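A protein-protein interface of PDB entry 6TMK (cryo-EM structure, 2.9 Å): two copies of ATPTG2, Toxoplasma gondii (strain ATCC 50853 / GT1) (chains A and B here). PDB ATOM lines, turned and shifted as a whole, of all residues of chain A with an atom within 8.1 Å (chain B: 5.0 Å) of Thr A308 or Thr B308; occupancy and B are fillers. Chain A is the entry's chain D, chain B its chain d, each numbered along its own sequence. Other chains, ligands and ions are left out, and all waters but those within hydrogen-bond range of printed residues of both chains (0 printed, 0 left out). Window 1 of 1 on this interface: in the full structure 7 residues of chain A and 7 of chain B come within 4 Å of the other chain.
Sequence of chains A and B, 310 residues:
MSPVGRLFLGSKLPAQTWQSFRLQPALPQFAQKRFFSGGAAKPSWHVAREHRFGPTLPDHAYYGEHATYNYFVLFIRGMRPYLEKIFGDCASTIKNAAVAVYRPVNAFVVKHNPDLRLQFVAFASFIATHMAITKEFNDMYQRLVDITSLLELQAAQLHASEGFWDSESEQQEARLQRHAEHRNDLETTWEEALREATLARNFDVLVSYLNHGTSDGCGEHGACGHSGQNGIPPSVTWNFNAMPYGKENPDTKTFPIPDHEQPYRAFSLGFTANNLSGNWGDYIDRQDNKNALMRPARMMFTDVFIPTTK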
ATOM      1  N   ARG A 295      20.811   3.072 -20.258  1.00  0.00           N
ATOM      2  CA  ARG A 295      20.213   4.400 -20.185  1.00  0.00           C
ATOM      3  C   ARG A 295      19.018   4.486 -19.246  1.00  0.00           C
ATOM      4  O   ARG A 295      18.902   5.499 -18.537  1.00  0.00           O
ATOM      5  CB  ARG A 295      19.820   4.848 -21.596  1.00  0.00           C
ATOM      6  CG  ARG A 295      20.918   5.573 -22.303  1.00  0.00           C
ATOM      7  CD  ARG A 295      20.652   5.775 -23.772  1.00  0.00           C
ATOM      8  NE  ARG A 295      21.864   5.578 -24.555  1.00  0.00           N
ATOM      9  CZ  ARG A 295      21.891   5.285 -25.846  1.00  0.00           C
ATOM     10  NH1 ARG A 295      20.774   5.154 -26.529  1.00  0.00           N
ATOM     11  NH2 ARG A 295      23.050   5.118 -26.446  1.00  0.00           N
ATOM     12  N   PRO A 296      18.115   3.510 -19.188  1.00  0.00           N
ATOM     13  CA  PRO A 296      17.041   3.578 -18.188  1.00  0.00           C
ATOM     14  C   PRO A 296      17.536   3.512 -16.750  1.00  0.00           C
ATOM     15  O   PRO A 296      16.812   3.942 -15.846  1.00  0.00           O
ATOM     16  CB  PRO A 296      16.160   2.375 -18.547  1.00  0.00           C
ATOM     17  CG  PRO A 296      16.415   2.145 -19.980  1.00  0.00           C
ATOM     18  CD  PRO A 296      17.847   2.479 -20.200  1.00  0.00           C
ATOM     19  N   ALA A 297      18.732   2.985 -16.507  1.00  0.00           N
ATOM     20  CA  ALA A 297      19.292   2.834 -15.168  1.00  0.00           C
ATOM     21  C   ALA A 297      20.521   3.716 -14.956  1.00  0.00           C
ATOM     22  O   ALA A 297      21.488   3.313 -14.312  1.00  0.00           O
ATOM     23  CB  ALA A 297      19.644   1.380 -14.900  1.00  0.00           C
ATOM     24  N   ARG A 298      20.484   4.941 -15.482  1.00  0.00           N
ATOM     25  CA  ARG A 298      21.617   5.849 -15.356  1.00  0.00           C
ATOM     26  C   ARG A 298      21.884   6.227 -13.908  1.00  0.00           C
ATOM     27  O   ARG A 298      23.032   6.478 -13.532  1.00  0.00           O
ATOM     28  CB  ARG A 298      21.340   7.099 -16.183  1.00  0.00           C
ATOM     29  CG  ARG A 298      22.511   8.010 -16.429  1.00  0.00           C
ATOM     30  CD  ARG A 298      22.005   9.334 -16.921  1.00  0.00           C
ATOM     31  NE  ARG A 298      21.168   9.152 -18.096  1.00  0.00           N
ATOM     32  CZ  ARG A 298      21.635   8.867 -19.305  1.00  0.00           C
ATOM     33  NH1 ARG A 298      22.936   8.748 -19.506  1.00  0.00           N
ATOM     34  NH2 ARG A 298      20.797   8.701 -20.314  1.00  0.00           N
ATOM     35  N   MET A 299      20.838   6.270 -13.089  1.00  0.00           N
ATOM     36  CA  MET A 299      20.981   6.624 -11.683  1.00  0.00           C
ATOM     37  C   MET A 299      21.930   5.687 -10.950  1.00  0.00           C
ATOM     38  O   MET A 299      22.544   6.079  -9.953  1.00  0.00           O
ATOM     39  CB  MET A 299      19.614   6.608 -11.025  1.00  0.00           C
ATOM     40  CG  MET A 299      19.545   7.283  -9.695  1.00  0.00           C
ATOM     41  SD  MET A 299      18.020   6.848  -8.859  1.00  0.00           S
ATOM     42  CE  MET A 299      17.961   8.166  -7.673  1.00  0.00           C
ATOM     43  N   PHE A 305      23.046  12.378  -7.903  1.00  0.00           N
ATOM     44  CA  PHE A 305      22.076  12.541  -8.973  1.00  0.00           C
ATOM     45  C   PHE A 305      21.127  13.663  -8.587  1.00  0.00           C
ATOM     46  O   PHE A 305      20.524  13.617  -7.511  1.00  0.00           O
ATOM     47  CB  PHE A 305      21.307  11.242  -9.225  1.00  0.00           C
ATOM     48  CG  PHE A 305      20.696  11.145 -10.583  1.00  0.00           C
ATOM     49  CD1 PHE A 305      19.383  11.501 -10.792  1.00  0.00           C
ATOM     50  CD2 PHE A 305      21.425  10.658 -11.647  1.00  0.00           C
ATOM     51  CE1 PHE A 305      18.828  11.402 -12.030  1.00  0.00           C
ATOM     52  CE2 PHE A 305      20.864  10.551 -12.891  1.00  0.00           C
ATOM     53  CZ  PHE A 305      19.566  10.917 -13.082  1.00  0.00           C
ATOM     54  N   ILE A 306      21.002  14.655  -9.455  1.00  0.00           N
ATOM     55  CA  ILE A 306      20.125  15.800  -9.252  1.00  0.00           C
ATOM     56  C   ILE A 306      19.075  15.798 -10.357  1.00  0.00           C
ATOM     57  O   ILE A 306      19.338  16.231 -11.478  1.00  0.00           O
ATOM     58  CB  ILE A 306      20.901  17.126  -9.227  1.00  0.00           C
ATOM     59  CG1 ILE A 306      21.770  17.215  -7.984  1.00  0.00           C
ATOM     60  CG2 ILE A 306      19.949  18.280  -9.245  1.00  0.00           C
ATOM     61  CD1 ILE A 306      22.944  18.070  -8.167  1.00  0.00           C
ATOM     62  N   PRO A 307      17.871  15.307 -10.081  1.00  0.00           N
ATOM     63  CA  PRO A 307      16.903  15.085 -11.157  1.00  0.00           C
ATOM     64  C   PRO A 307      16.351  16.381 -11.725  1.00  0.00           C
ATOM     65  O   PRO A 307      16.599  17.486 -11.239  1.00  0.00           O
ATOM     66  CB  PRO A 307      15.788  14.301 -10.463  1.00  0.00           C
ATOM     67  CG  PRO A 307      16.390  13.762  -9.248  1.00  0.00           C
ATOM     68  CD  PRO A 307      17.355  14.791  -8.809  1.00  0.00           C
ATOM     69  N   THR A 308      15.568  16.209 -12.782  1.00  0.00           N
ATOM     70  CA  THR A 308      14.943  17.312 -13.481  1.00  0.00           C
ATOM     71  C   THR A 308      13.867  17.970 -12.629  1.00  0.00           C
ATOM     72  O   THR A 308      13.428  17.451 -11.601  1.00  0.00           O
ATOM     73  CB  THR A 308      14.294  16.834 -14.772  1.00  0.00           C
ATOM     74  OG1 THR A 308      13.264  15.891 -14.458  1.00  0.00           O
ATOM     75  CG2 THR A 308      15.297  16.186 -15.659  1.00  0.00           C
ATOM     76  N   THR A 309      13.435  19.133 -13.093  1.00  0.00           N
ATOM     77  CA  THR A 309      12.289  19.841 -12.552  1.00  0.00           C
ATOM     78  C   THR A 309      11.130  19.705 -13.527  1.00  0.00           C
ATOM     79  O   THR A 309      11.277  20.008 -14.716  1.00  0.00           O
ATOM     80  CB  THR A 309      12.619  21.316 -12.325  1.00  0.00           C
ATOM     81  OG1 THR A 309      13.732  21.431 -11.427  1.00  0.00           O
ATOM     82  CG2 THR A 309      11.436  22.038 -11.761  1.00  0.00           C
ATOM     83  N   LYS A 310       9.988  19.239 -13.037  1.00  0.00           N
ATOM     84  CA  LYS A 310       8.830  19.040 -13.908  1.00  0.00           C
ATOM     85  C   LYS A 310       7.502  19.180 -13.164  1.00  0.00           C
ATOM     86  O   LYS A 310       7.204  18.435 -12.233  1.00  0.00           O
ATOM     87  CB  LYS A 310       8.906  17.678 -14.588  1.00  0.00           C
ATOM     88  CG  LYS A 310       8.048  17.559 -15.842  1.00  0.00           C
ATOM     89  CD  LYS A 310       8.785  18.064 -17.075  1.00  0.00           C
ATOM     90  CE  LYS A 310       7.848  18.280 -18.257  1.00  0.00           C
ATOM     91  NZ  LYS A 310       6.959  19.470 -18.113  1.00  0.00           N
ATOM     92  OXT LYS A 310       6.689  20.043 -13.489  1.00  0.00           O
ATOM     93  N   ILE B 306      12.254   7.344  -9.950  1.00  0.00           N
ATOM     94  CA  ILE B 306      12.723   6.762 -11.198  1.00  0.00           C
ATOM     95  C   ILE B 306      12.950   7.889 -12.196  1.00  0.00           C
ATOM     96  O   ILE B 306      12.008   8.386 -12.813  1.00  0.00           O
ATOM     97  CB  ILE B 306      11.741   5.718 -11.754  1.00  0.00           C
ATOM     98  CG1 ILE B 306      11.705   4.489 -10.862  1.00  0.00           C
ATOM     99  CG2 ILE B 306      12.146   5.313 -13.136  1.00  0.00           C
ATOM    100  CD1 ILE B 306      10.431   3.771 -10.927  1.00  0.00           C
ATOM    101  N   PRO B 307      14.190   8.332 -12.377  1.00  0.00           N
ATOM    102  CA  PRO B 307      14.433   9.547 -13.156  1.00  0.00           C
ATOM    103  C   PRO B 307      14.180   9.349 -14.641  1.00  0.00           C
ATOM    104  O   PRO B 307      13.925   8.253 -15.139  1.00  0.00           O
ATOM    105  CB  PRO B 307      15.916   9.827 -12.910  1.00  0.00           C
ATOM    106  CG  PRO B 307      16.261   9.071 -11.710  1.00  0.00           C
ATOM    107  CD  PRO B 307      15.438   7.846 -11.778  1.00  0.00           C
ATOM    108  N   THR B 308      14.277  10.467 -15.350  1.00  0.00           N
ATOM    109  CA  THR B 308      14.067  10.507 -16.782  1.00  0.00           C
ATOM    110  C   THR B 308      15.184   9.790 -17.527  1.00  0.00           C
ATOM    111  O   THR B 308      16.240   9.463 -16.980  1.00  0.00           O
ATOM    112  CB  THR B 308      14.017  11.945 -17.279  1.00  0.00           C
ATOM    113  OG1 THR B 308      15.273  12.575 -17.015  1.00  0.00           O
ATOM    114  CG2 THR B 308      12.933  12.701 -16.598  1.00  0.00           C
ATOM    115  N   THR B 309      14.931   9.560 -18.806  1.00  0.00           N
ATOM    116  CA  THR B 309      15.922   9.066 -19.746  1.00  0.00           C
ATOM    117  C   THR B 309      16.343  10.212 -20.654  1.00  0.00           C
ATOM    118  O   THR B 309      15.492  10.870 -21.261  1.00  0.00           O
ATOM    119  CB  THR B 309      15.357   7.913 -20.575  1.00  0.00           C
ATOM    120  OG1 THR B 309      14.934   6.852 -19.706  1.00  0.00           O
ATOM    121  CG2 THR B 309      16.385   7.403 -21.534  1.00  0.00           C
ATOM    122  N   LYS B 310      17.643  10.459 -20.737  1.00  0.00           N
ATOM    123  CA  LYS B 310      18.142  11.561 -21.559  1.00  0.00           C
ATOM    124  C   LYS B 310      19.551  11.308 -22.095  1.00  0.00           C
ATOM    125  O   LYS B 310      20.508  11.147 -21.340  1.00  0.00           O
ATOM    126  CB  LYS B 310      18.111  12.866 -20.771  1.00  0.00           C
ATOM    127  CG  LYS B 310      18.141  14.119 -21.638  1.00  0.00           C
ATOM    128  CD  LYS B 310      16.743  14.522 -22.089  1.00  0.00           C
ATOM    129  CE  LYS B 310      16.774  15.541 -23.223  1.00  0.00           C
ATOM    130  NZ  LYS B 310      17.200  14.971 -24.535  1.00  0.00           N
ATOM    131  OXT LYS B 310      19.764  11.269 -23.306  1.00  0.00           O
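Phe A305 touches Pro B307 (CE1 to CB, 3.4 Å).
Thr A308 touches Thr B308.
Of the 5 printed residues of chain B, 3 touch a printed residue of chain A.
Along chain B the printed residues that touch a printed residue of chain A span positions 307 to 310.
Hydrophobic or aromatic side chains of chain A that line the printed part of chain B: Phe A305.
Among the printed residues, 3 pairs touch across the chains.
Among the printed residues, no Asp or Glu carboxylate lies within 4 Å of a Lys or Arg side-chain nitrogen of the other chain.
The guanidinium group of Arg A298 is in salt-bridge range of the chain-end carboxylate of Lys B310, at 2.7 Å.
Thr A308 touches its own counterpart, Thr B308.
Thr A308 touches one residue of chain B.
Thr B308 touches just one residue of chain A: Thr A308.
Of the printed residues of chain B, Arg A298 touches Lys B310.
Of the printed residues of chain B, Phe A305 touches Pro B307.
Printed residues of chain A within 4 Å of Pro B307: Phe A305 (3.4 Å).
Printed residues of chain A within 4 Å of Lys B310: Arg A298.
The nearest printed residue of chain B that does not touch Thr A308 is Pro B307 (6.4 Å).
The nearest printed residue of chain A that does not touch Lys B310 is Arg A295 (5.6 Å).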
